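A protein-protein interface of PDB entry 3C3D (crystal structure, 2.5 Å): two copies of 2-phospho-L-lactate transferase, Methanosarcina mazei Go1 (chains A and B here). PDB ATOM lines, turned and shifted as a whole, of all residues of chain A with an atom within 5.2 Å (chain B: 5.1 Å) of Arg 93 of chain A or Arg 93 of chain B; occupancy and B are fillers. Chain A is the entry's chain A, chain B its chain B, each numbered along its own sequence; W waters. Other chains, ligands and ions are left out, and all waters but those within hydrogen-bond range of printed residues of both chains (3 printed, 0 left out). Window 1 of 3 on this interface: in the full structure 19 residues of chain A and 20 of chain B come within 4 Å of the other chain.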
ATOM      1  N   SER A  39       2.811 -14.928  17.001  1.00  0.00           N
ATOM      2  CA  SER A  39       2.537 -14.775  18.415  1.00  0.00           C
ATOM      3  C   SER A  39       2.465 -16.109  19.157  1.00  0.00           C
ATOM      4  O   SER A  39       1.556 -16.331  19.951  1.00  0.00           O
ATOM      5  CB  SER A  39       1.231 -14.019  18.608  1.00  0.00           C
ATOM      6  OG  SER A  39       1.314 -12.747  17.997  1.00  0.00           O
ATOM      7  N   ASN A  41       1.800 -19.133  18.008  1.00  0.00           N
ATOM      8  CA  ASN A  41       0.917 -20.175  17.515  1.00  0.00           C
ATOM      9  C   ASN A  41       0.781 -20.222  16.007  1.00  0.00           C
ATOM     10  O   ASN A  41       0.802 -19.197  15.332  1.00  0.00           O
ATOM     11  CB  ASN A  41      -0.452 -20.022  18.178  1.00  0.00           C
ATOM     12  CG  ASN A  41      -0.383 -20.228  19.676  1.00  0.00           C
ATOM     13  OD1 ASN A  41      -0.163 -21.343  20.147  1.00  0.00           O
ATOM     14  ND2 ASN A  41      -0.552 -19.151  20.435  1.00  0.00           N
ATOM     15  N   THR A  73      -7.220  -8.890  22.630  1.00  0.00           N
ATOM     16  CA  THR A  73      -5.774  -8.929  22.623  1.00  0.00           C
ATOM     17  C   THR A  73      -5.137  -8.062  21.539  1.00  0.00           C
ATOM     18  O   THR A  73      -4.157  -7.359  21.780  1.00  0.00           O
ATOM     19  CB  THR A  73      -5.312 -10.354  22.480  1.00  0.00           C
ATOM     20  OG1 THR A  73      -5.715 -11.075  23.643  1.00  0.00           O
ATOM     21  CG2 THR A  73      -3.805 -10.424  22.321  1.00  0.00           C
ATOM     22  N   TYR A  74      -5.714  -8.125  20.349  1.00  0.00           N
ATOM     23  CA  TYR A  74      -5.216  -7.360  19.224  1.00  0.00           C
ATOM     24  C   TYR A  74      -5.264  -5.866  19.525  1.00  0.00           C
ATOM     25  O   TYR A  74      -4.316  -5.139  19.238  1.00  0.00           O
ATOM     26  CB  TYR A  74      -6.058  -7.641  17.986  1.00  0.00           C
ATOM     27  CG  TYR A  74      -5.637  -6.842  16.774  1.00  0.00           C
ATOM     28  CD1 TYR A  74      -4.511  -7.210  16.038  1.00  0.00           C
ATOM     29  CD2 TYR A  74      -6.352  -5.714  16.376  1.00  0.00           C
ATOM     30  CE1 TYR A  74      -4.107  -6.470  14.929  1.00  0.00           C
ATOM     31  CE2 TYR A  74      -5.960  -4.967  15.273  1.00  0.00           C
ATOM     32  CZ  TYR A  74      -4.836  -5.350  14.552  1.00  0.00           C
ATOM     33  OH  TYR A  74      -4.438  -4.613  13.452  1.00  0.00           O
ATOM     34  N   GLU A  84       0.808  -7.427  15.360  1.00  0.00           N
ATOM     35  CA  GLU A  84       1.076  -8.864  15.286  1.00  0.00           C
ATOM     36  C   GLU A  84       1.403  -9.260  13.857  1.00  0.00           C
ATOM     37  O   GLU A  84       2.113 -10.237  13.628  1.00  0.00           O
ATOM     38  CB  GLU A  84      -0.112  -9.696  15.777  1.00  0.00           C
ATOM     39  CG  GLU A  84      -0.439  -9.507  17.239  1.00  0.00           C
ATOM     40  CD  GLU A  84      -1.441 -10.531  17.761  1.00  0.00           C
ATOM     41  OE1 GLU A  84      -1.021 -11.651  18.129  1.00  0.00           O
ATOM     42  OE2 GLU A  84      -2.653 -10.215  17.798  1.00  0.00           O
ATOM     43  N   LEU A  88      -5.820 -10.485  14.475  1.00  0.00           N
ATOM     44  CA  LEU A  88      -6.170 -11.761  15.093  1.00  0.00           C
ATOM     45  C   LEU A  88      -7.281 -11.648  16.126  1.00  0.00           C
ATOM     46  O   LEU A  88      -7.071 -11.056  17.182  1.00  0.00           O
ATOM     47  CB  LEU A  88      -4.946 -12.363  15.770  1.00  0.00           C
ATOM     48  CG  LEU A  88      -4.298 -13.574  15.108  1.00  0.00           C
ATOM     49  CD1 LEU A  88      -4.277 -13.382  13.601  1.00  0.00           C
ATOM     50  CD2 LEU A  88      -2.891 -13.772  15.658  1.00  0.00           C
ATOM     51  N   GLY A  89      -8.450 -12.215  15.827  1.00  0.00           N
ATOM     52  CA  GLY A  89      -9.554 -12.168  16.766  1.00  0.00           C
ATOM     53  C   GLY A  89      -9.361 -13.150  17.913  1.00  0.00           C
ATOM     54  O   GLY A  89      -8.619 -14.125  17.780  1.00  0.00           O
ATOM     55  N   ASP A  90     -10.031 -12.908  19.039  1.00  0.00           N
ATOM     56  CA  ASP A  90      -9.895 -13.779  20.200  1.00  0.00           C
ATOM     57  C   ASP A  90     -10.372 -15.206  19.942  1.00  0.00           C
ATOM     58  O   ASP A  90      -9.680 -16.162  20.297  1.00  0.00           O
ATOM     59  CB  ASP A  90     -10.630 -13.179  21.420  1.00  0.00           C
ATOM     60  CG  ASP A  90     -10.209 -11.731  21.713  1.00  0.00           C
ATOM     61  OD1 ASP A  90      -8.993 -11.422  21.639  1.00  0.00           O
ATOM     62  OD2 ASP A  90     -11.096 -10.905  22.020  1.00  0.00           O
ATOM     63  N   ARG A  91     -11.542 -15.360  19.323  1.00  0.00           N
ATOM     64  CA  ARG A  91     -12.062 -16.699  19.035  1.00  0.00           C
ATOM     65  C   ARG A  91     -11.184 -17.437  18.027  1.00  0.00           C
ATOM     66  O   ARG A  91     -10.933 -18.642  18.161  1.00  0.00           O
ATOM     67  CB  ARG A  91     -13.513 -16.610  18.551  1.00  0.00           C
ATOM     68  CG  ARG A  91     -14.464 -16.119  19.641  1.00  0.00           C
ATOM     69  CD  ARG A  91     -15.893 -15.893  19.144  1.00  0.00           C
ATOM     70  NE  ARG A  91     -16.593 -17.141  18.858  1.00  0.00           N
ATOM     71  CZ  ARG A  91     -17.042 -17.986  19.785  1.00  0.00           C
ATOM     72  NH1 ARG A  91     -17.669 -19.103  19.426  1.00  0.00           N
ATOM     73  NH2 ARG A  91     -16.873 -17.711  21.073  1.00  0.00           N
ATOM     74  N   ASP A  92     -10.701 -16.704  17.031  1.00  0.00           N
ATOM     75  CA  ASP A  92      -9.833 -17.251  15.995  1.00  0.00           C
ATOM     76  C   ASP A  92      -8.524 -17.746  16.621  1.00  0.00           C
ATOM     77  O   ASP A  92      -8.006 -18.808  16.252  1.00  0.00           O
ATOM     78  CB  ASP A  92      -9.538 -16.157  14.970  1.00  0.00           C
ATOM     79  CG  ASP A  92      -8.713 -16.651  13.801  1.00  0.00           C
ATOM     80  OD1 ASP A  92      -7.926 -15.852  13.259  1.00  0.00           O
ATOM     81  OD2 ASP A  92      -8.859 -17.823  13.406  1.00  0.00           O
ATOM     82  N   ARG A  93      -7.990 -16.983  17.578  1.00  0.00           N
ATOM     83  CA  ARG A  93      -6.735 -17.354  18.235  1.00  0.00           C
ATOM     84  C   ARG A  93      -6.881 -18.696  18.953  1.00  0.00           C
ATOM     85  O   ARG A  93      -5.902 -19.446  19.086  1.00  0.00           O
ATOM     86  CB  ARG A  93      -6.281 -16.261  19.226  1.00  0.00           C
ATOM     87  CG  ARG A  93      -4.789 -16.331  19.599  1.00  0.00           C
ATOM     88  CD  ARG A  93      -4.391 -15.358  20.742  1.00  0.00           C
ATOM     89  NE  ARG A  93      -4.605 -13.956  20.381  1.00  0.00           N
ATOM     90  CZ  ARG A  93      -3.740 -13.209  19.698  1.00  0.00           C
ATOM     91  NH1 ARG A  93      -2.574 -13.711  19.292  1.00  0.00           N
ATOM     92  NH2 ARG A  93      -4.053 -11.957  19.404  1.00  0.00           N
ATOM     93  N   ALA A  94      -8.097 -19.009  19.406  1.00  0.00           N
ATOM     94  CA  ALA A  94      -8.343 -20.278  20.095  1.00  0.00           C
ATOM     95  C   ALA A  94      -8.035 -21.451  19.163  1.00  0.00           C
ATOM     96  O   ALA A  94      -7.512 -22.487  19.596  1.00  0.00           O
ATOM     97  CB  ALA A  94      -9.781 -20.347  20.565  1.00  0.00           C
ATOM     98  N   THR A  95      -8.344 -21.266  17.880  1.00  0.00           N
ATOM     99  CA  THR A  95      -8.101 -22.279  16.857  1.00  0.00           C
ATOM    100  C   THR A  95      -6.595 -22.496  16.710  1.00  0.00           C
ATOM    101  O   THR A  95      -6.123 -23.635  16.656  1.00  0.00           O
ATOM    102  CB  THR A  95      -8.708 -21.831  15.501  1.00  0.00           C
ATOM    103  OG1 THR A  95     -10.107 -21.574  15.681  1.00  0.00           O
ATOM    104  CG2 THR A  95      -8.523 -22.910  14.419  1.00  0.00           C
ATOM    105  N   HIS A  96      -5.838 -21.404  16.656  1.00  0.00           N
ATOM    106  CA  HIS A  96      -4.384 -21.491  16.533  1.00  0.00           C
ATOM    107  C   HIS A  96      -3.809 -22.215  17.763  1.00  0.00           C
ATOM    108  O   HIS A  96      -2.925 -23.072  17.640  1.00  0.00           O
ATOM    109  CB  HIS A  96      -3.767 -20.090  16.442  1.00  0.00           C
ATOM    110  CG  HIS A  96      -4.439 -19.187  15.455  1.00  0.00           C
ATOM    111  ND1 HIS A  96      -4.310 -17.816  15.495  1.00  0.00           N
ATOM    112  CD2 HIS A  96      -5.248 -19.456  14.401  1.00  0.00           C
ATOM    113  CE1 HIS A  96      -5.011 -17.279  14.512  1.00  0.00           C
ATOM    114  NE2 HIS A  96      -5.590 -18.252  13.834  1.00  0.00           N
ATOM    115  N   ILE A  97      -4.312 -21.873  18.946  1.00  0.00           N
ATOM    116  CA  ILE A  97      -3.826 -22.495  20.172  1.00  0.00           C
ATOM    117  C   ILE A  97      -4.116 -24.007  20.219  1.00  0.00           C
ATOM    118  O   ILE A  97      -3.191 -24.818  20.430  1.00  0.00           O
ATOM    119  CB  ILE A  97      -4.420 -21.772  21.421  1.00  0.00           C
ATOM    120  CG1 ILE A  97      -3.937 -20.312  21.431  1.00  0.00           C
ATOM    121  CG2 ILE A  97      -3.987 -22.465  22.693  1.00  0.00           C
ATOM    122  CD1 ILE A  97      -4.676 -19.406  22.407  1.00  0.00           C
ATOM    123  N   ILE A  98      -5.376 -24.391  20.006  1.00  0.00           N
ATOM    124  CA  ILE A  98      -5.754 -25.805  20.008  1.00  0.00           C
ATOM    125  C   ILE A  98      -4.887 -26.564  19.014  1.00  0.00           C
ATOM    126  O   ILE A  98      -4.374 -27.647  19.314  1.00  0.00           O
ATOM    127  CB  ILE A  98      -7.244 -25.989  19.615  1.00  0.00           C
ATOM    128  CG1 ILE A  98      -8.132 -25.401  20.703  1.00  0.00           C
ATOM    129  CG2 ILE A  98      -7.574 -27.467  19.431  1.00  0.00           C
ATOM    130  CD1 ILE A  98      -9.551 -25.250  20.268  1.00  0.00           C
ATOM    131  N   SER B  39      -0.052 -22.077  26.075  1.00  0.00           N
ATOM    132  CA  SER B  39      -0.646 -21.688  24.809  1.00  0.00           C
ATOM    133  C   SER B  39       0.330 -20.932  23.908  1.00  0.00           C
ATOM    134  O   SER B  39      -0.022 -19.947  23.263  1.00  0.00           O
ATOM    135  CB  SER B  39      -1.906 -20.874  25.068  1.00  0.00           C
ATOM    136  OG  SER B  39      -2.817 -21.650  25.833  1.00  0.00           O
ATOM    137  N   THR B  73     -10.787 -15.565  24.234  1.00  0.00           N
ATOM    138  CA  THR B  73     -10.114 -16.806  23.885  1.00  0.00           C
ATOM    139  C   THR B  73     -10.356 -17.892  24.924  1.00  0.00           C
ATOM    140  O   THR B  73     -10.645 -19.041  24.582  1.00  0.00           O
ATOM    141  CB  THR B  73      -8.593 -16.588  23.714  1.00  0.00           C
ATOM    142  OG1 THR B  73      -8.364 -15.664  22.650  1.00  0.00           O
ATOM    143  CG2 THR B  73      -7.901 -17.888  23.380  1.00  0.00           C
ATOM    144  N   TYR B  74     -10.241 -17.521  26.193  1.00  0.00           N
ATOM    145  CA  TYR B  74     -10.445 -18.469  27.275  1.00  0.00           C
ATOM    146  C   TYR B  74     -11.841 -19.089  27.246  1.00  0.00           C
ATOM    147  O   TYR B  74     -11.996 -20.293  27.445  1.00  0.00           O
ATOM    148  CB  TYR B  74     -10.246 -17.783  28.623  1.00  0.00           C
ATOM    149  CG  TYR B  74     -10.391 -18.733  29.780  1.00  0.00           C
ATOM    150  CD1 TYR B  74      -9.370 -19.630  30.090  1.00  0.00           C
ATOM    151  CD2 TYR B  74     -11.560 -18.764  30.540  1.00  0.00           C
ATOM    152  CE1 TYR B  74      -9.505 -20.537  31.132  1.00  0.00           C
ATOM    153  CE2 TYR B  74     -11.709 -19.668  31.586  1.00  0.00           C
ATOM    154  CZ  TYR B  74     -10.674 -20.550  31.874  1.00  0.00           C
ATOM    155  OH  TYR B  74     -10.788 -21.445  32.912  1.00  0.00           O
ATOM    156  N   GLU B  84      -6.977 -24.098  29.493  1.00  0.00           N
ATOM    157  CA  GLU B  84      -5.600 -23.609  29.375  1.00  0.00           C
ATOM    158  C   GLU B  84      -4.798 -23.879  30.640  1.00  0.00           C
ATOM    159  O   GLU B  84      -3.571 -23.848  30.613  1.00  0.00           O
ATOM    160  CB  GLU B  84      -5.546 -22.109  29.068  1.00  0.00           C
ATOM    161  CG  GLU B  84      -6.257 -21.690  27.796  1.00  0.00           C
ATOM    162  CD  GLU B  84      -5.847 -20.301  27.302  1.00  0.00           C
ATOM    163  OE1 GLU B  84      -4.808 -20.190  26.616  1.00  0.00           O
ATOM    164  OE2 GLU B  84      -6.568 -19.320  27.605  1.00  0.00           O
ATOM    165  N   LEU B  88      -6.772 -17.114  31.560  1.00  0.00           N
ATOM    166  CA  LEU B  88      -5.979 -16.156  30.802  1.00  0.00           C
ATOM    167  C   LEU B  88      -6.851 -15.100  30.141  1.00  0.00           C
ATOM    168  O   LEU B  88      -7.599 -15.413  29.224  1.00  0.00           O
ATOM    169  CB  LEU B  88      -5.197 -16.885  29.714  1.00  0.00           C
ATOM    170  CG  LEU B  88      -3.686 -17.021  29.865  1.00  0.00           C
ATOM    171  CD1 LEU B  88      -3.371 -17.539  31.259  1.00  0.00           C
ATOM    172  CD2 LEU B  88      -3.136 -17.960  28.800  1.00  0.00           C
ATOM    173  N   GLY B  89      -6.752 -13.852  30.588  1.00  0.00           N
ATOM    174  CA  GLY B  89      -7.544 -12.794  29.985  1.00  0.00           C
ATOM    175  C   GLY B  89      -6.945 -12.330  28.668  1.00  0.00           C
ATOM    176  O   GLY B  89      -5.778 -12.572  28.388  1.00  0.00           O
ATOM    177  N   ASP B  90      -7.728 -11.639  27.854  1.00  0.00           N
ATOM    178  CA  ASP B  90      -7.221 -11.188  26.563  1.00  0.00           C
ATOM    179  C   ASP B  90      -6.110 -10.145  26.653  1.00  0.00           C
ATOM    180  O   ASP B  90      -5.106 -10.249  25.950  1.00  0.00           O
ATOM    181  CB  ASP B  90      -8.382 -10.685  25.707  1.00  0.00           C
ATOM    182  CG  ASP B  90      -9.471 -11.732  25.555  1.00  0.00           C
ATOM    183  OD1 ASP B  90      -9.123 -12.908  25.304  1.00  0.00           O
ATOM    184  OD2 ASP B  90     -10.666 -11.387  25.688  1.00  0.00           O
ATOM    185  N   ARG B  91      -6.274  -9.152  27.520  1.00  0.00           N
ATOM    186  CA  ARG B  91      -5.255  -8.119  27.672  1.00  0.00           C
ATOM    187  C   ARG B  91      -4.010  -8.707  28.323  1.00  0.00           C
ATOM    188  O   ARG B  91      -2.877  -8.372  27.960  1.00  0.00           O
ATOM    189  CB  ARG B  91      -5.807  -6.950  28.499  1.00  0.00           C
ATOM    190  CG  ARG B  91      -6.958  -6.218  27.802  1.00  0.00           C
ATOM    191  CD  ARG B  91      -7.633  -5.183  28.697  1.00  0.00           C
ATOM    192  NE  ARG B  91      -6.831  -3.976  28.857  1.00  0.00           N
ATOM    193  CZ  ARG B  91      -6.626  -3.075  27.898  1.00  0.00           C
ATOM    194  NH1 ARG B  91      -5.875  -2.008  28.144  1.00  0.00           N
ATOM    195  NH2 ARG B  91      -7.178  -3.234  26.696  1.00  0.00           N
ATOM    196  N   ASP B  92      -4.223  -9.612  29.267  1.00  0.00           N
ATOM    197  CA  ASP B  92      -3.123 -10.249  29.954  1.00  0.00           C
ATOM    198  C   ASP B  92      -2.284 -11.066  28.962  1.00  0.00           C
ATOM    199  O   ASP B  92      -1.052 -11.142  29.084  1.00  0.00           O
ATOM    200  CB  ASP B  92      -3.675 -11.148  31.055  1.00  0.00           C
ATOM    201  CG  ASP B  92      -2.586 -11.787  31.887  1.00  0.00           C
ATOM    202  OD1 ASP B  92      -2.724 -12.996  32.179  1.00  0.00           O
ATOM    203  OD2 ASP B  92      -1.603 -11.097  32.255  1.00  0.00           O
ATOM    204  N   ARG B  93      -2.949 -11.672  27.975  1.00  0.00           N
ATOM    205  CA  ARG B  93      -2.264 -12.488  26.975  1.00  0.00           C
ATOM    206  C   ARG B  93      -1.311 -11.629  26.142  1.00  0.00           C
ATOM    207  O   ARG B  93      -0.245 -12.097  25.725  1.00  0.00           O
ATOM    208  CB  ARG B  93      -3.278 -13.199  26.046  1.00  0.00           C
ATOM    209  CG  ARG B  93      -2.690 -14.410  25.275  1.00  0.00           C
ATOM    210  CD  ARG B  93      -3.702 -15.056  24.314  1.00  0.00           C
ATOM    211  NE  ARG B  93      -4.889 -15.579  24.995  1.00  0.00           N
ATOM    212  CZ  ARG B  93      -4.970 -16.778  25.568  1.00  0.00           C
ATOM    213  NH1 ARG B  93      -3.933 -17.606  25.539  1.00  0.00           N
ATOM    214  NH2 ARG B  93      -6.093 -17.132  26.196  1.00  0.00           N
ATOM    215  N   ALA B  94      -1.695 -10.376  25.906  1.00  0.00           N
ATOM    216  CA  ALA B  94      -0.857  -9.469  25.130  1.00  0.00           C
ATOM    217  C   ALA B  94       0.532  -9.360  25.754  1.00  0.00           C
ATOM    218  O   ALA B  94       1.547  -9.377  25.043  1.00  0.00           O
ATOM    219  CB  ALA B  94      -1.509  -8.092  25.035  1.00  0.00           C
ATOM    220  N   THR B  95       0.575  -9.275  27.079  1.00  0.00           N
ATOM    221  CA  THR B  95       1.836  -9.186  27.811  1.00  0.00           C
ATOM    222  C   THR B  95       2.692 -10.432  27.536  1.00  0.00           C
ATOM    223  O   THR B  95       3.895 -10.332  27.282  1.00  0.00           O
ATOM    224  CB  THR B  95       1.573  -9.086  29.340  1.00  0.00           C
ATOM    225  OG1 THR B  95       0.721  -7.965  29.598  1.00  0.00           O
ATOM    226  CG2 THR B  95       2.879  -8.919  30.116  1.00  0.00           C
ATOM    227  N   HIS B  96       2.058 -11.604  27.597  1.00  0.00           N
ATOM    228  CA  HIS B  96       2.746 -12.871  27.354  1.00  0.00           C
ATOM    229  C   HIS B  96       3.330 -12.878  25.949  1.00  0.00           C
ATOM    230  O   HIS B  96       4.467 -13.294  25.734  1.00  0.00           O
ATOM    231  CB  HIS B  96       1.765 -14.040  27.468  1.00  0.00           C
ATOM    232  CG  HIS B  96       1.011 -14.077  28.760  1.00  0.00           C
ATOM    233  ND1 HIS B  96      -0.109 -14.859  28.943  1.00  0.00           N
ATOM    234  CD2 HIS B  96       1.207 -13.414  29.925  1.00  0.00           C
ATOM    235  CE1 HIS B  96      -0.573 -14.673  30.166  1.00  0.00           C
ATOM    236  NE2 HIS B  96       0.207 -13.803  30.780  1.00  0.00           N
ATOM    237  N   ILE B  97       2.524 -12.428  24.997  1.00  0.00           N
ATOM    238  CA  ILE B  97       2.925 -12.394  23.608  1.00  0.00           C
ATOM    239  C   ILE B  97       4.072 -11.415  23.365  1.00  0.00           C
ATOM    240  O   ILE B  97       5.087 -11.786  22.765  1.00  0.00           O
ATOM    241  CB  ILE B  97       1.714 -12.035  22.709  1.00  0.00           C
ATOM    242  CG1 ILE B  97       0.681 -13.172  22.779  1.00  0.00           C
ATOM    243  CG2 ILE B  97       2.174 -11.775  21.277  1.00  0.00           C
ATOM    244  CD1 ILE B  97      -0.630 -12.880  22.062  1.00  0.00           C
ATOM    245  N   ILE B  98       3.924 -10.175  23.835  1.00  0.00           N
ATOM    246  CA  ILE B  98       4.979  -9.180  23.654  1.00  0.00           C
ATOM    247  C   ILE B  98       6.292  -9.688  24.254  1.00  0.00           C
ATOM    248  O   ILE B  98       7.356  -9.563  23.646  1.00  0.00           O
ATOM    249  CB  ILE B  98       4.586  -7.828  24.296  1.00  0.00           C
ATOM    250  CG1 ILE B  98       3.382  -7.243  23.557  1.00  0.00           C
ATOM    251  CG2 ILE B  98       5.742  -6.843  24.225  1.00  0.00           C
ATOM    252  CD1 ILE B  98       2.758  -6.072  24.274  1.00  0.00           C
HETATM  253  O   HOH W   1      -6.963 -13.144  21.407  1.00  0.00           O
HETATM  254  O   HOH W   2     -12.801  -9.816  23.929  1.00  0.00           O
HETATM  255  O   HOH W   3      -6.705 -13.676  24.390  1.00  0.00           O
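The side-chain amide nitrogen (ND2) of Asn 41 of chain A is in hydrogen-bond range of the backbone carbonyl oxygen (O) of Ser 39 of chain B (3.0 Å). O of Asp 90 of chain B is in hydrogen-bond range of OG1 of Thr 73 of chain A. The side-chain hydroxyl (OG1) of Thr 73 of chain B sits at hydrogen-bond distance from the backbone carbonyl oxygen (O) of Asp 90 of chain A.
The side-chain hydroxyl (OG) of Ser 39 of chain A sits at hydrogen-bond distance from the side-chain carboxylate (OE1) of Glu 84 of chain A. OD1 of Asp 90 of chain A sits at hydrogen-bond distance from N of Thr 73 of chain A, at 3.2 Å. The guanidinium group (NH2) of Arg 93 of chain A lies within salt-bridge range of the side-chain carboxylate (OE2) of Glu 84 of chain A, at 2.8 Å. OE1 of Glu 84 of chain B lies within hydrogen-bond range of OG of Ser 39 of chain B, at 2.6 Å. The backbone NH (N) of Thr 73 of chain B is in hydrogen-bond range of the side-chain carboxylate (OD1) of Asp 90 of chain B (3.3 Å). The side-chain carboxylate of Glu 84 of chain B lies within salt-bridge range of the guanidinium group of Arg 93 of chain B (2.6 Å).
Among the printed residues, merely in contact across the chains: Ile 97 of chain A with Ser 39 of chain B (3.4 Å), Arg 93 of chain A with Ile 97 of chain B (3.5 Å), Ser 39 of chain A with Ile 97 of chain B (3.5 Å), Arg 93 of chain A with Arg 93 of chain B (3.7 Å), Ile 97 of chain A with Arg 93 of chain B (3.7 Å), Ile 97 of chain A with Thr 73 of chain B (3.7 Å) and Asp 90 of chain A with Asp 90 of chain B (3.7 Å).
Of the printed residues of chain B, Thr 73 of chain A touches Asp 90 (2.5 Å). Arg 93 of chain A touches just these residues of chain B: Arg 93 and Ile 97. Of the printed residues of chain A, Thr 73 of chain B touches Asp 90 and Ile 97. Of the printed residues of chain A, Asp 90 of chain B touches Thr 73 and Asp 90. Arg 93 of chain B touches two residues of chain A. The nearest residue of chain A that does not touch Arg 93 of chain B is Thr 73 of chain A (4.03 Å).
Printed residues of chain A that touch a printed residue of chain B: Ser 39, Asn 41, Thr 73, Asp 90, Arg 93 and Ile 97. Printed residues of chain B that touch a printed residue of chain A: Ser 39, Thr 73, Asp 90, Arg 93 and Ile 97. Among the printed residues, 10 pairs touch across the chains.
Ser 39 of chain A touches Ile 97 of chain B, and with the chains exchanged Ile 97 of chain A touches Ser 39 of chain B. Thr 73 of chain A touches Asp 90 of chain B, and with the chains exchanged Asp 90 of chain A touches Thr 73 of chain B. Arg 93 of chain A touches its own counterpart, Arg 93 of chain B. Arg 93 of chain A touches Ile 97 of chain B, and with the chains exchanged Ile 97 of chain A touches Arg 93 of chain B. 15 positions are printed for both chains.
Water W1 lies within hydrogen-bond range of OD1 of Asp 90 of chain A (2.7 Å), NE of Arg 93 of chain A (2.7 Å), OG1 of Thr 73 of chain B (3.1 Å) and OG1 of Thr 73 of chain A (3.3 Å). Water W3 lies within hydrogen-bond range of the side-chain carboxylate of Asp 90 of chain B (2.7 Å), the guanidinium group of Arg 93 of chain B (2.7 Å), the side-chain hydroxyl of Thr 73 of chain A (2.9 Å) and the side-chain hydroxyl of Thr 73 of chain B (3.1 Å). Water W2 bridges OD2 of Asp 90 of chain A (2.8 Å) and OD2 of Asp 90 of chain B (3.2 Å).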
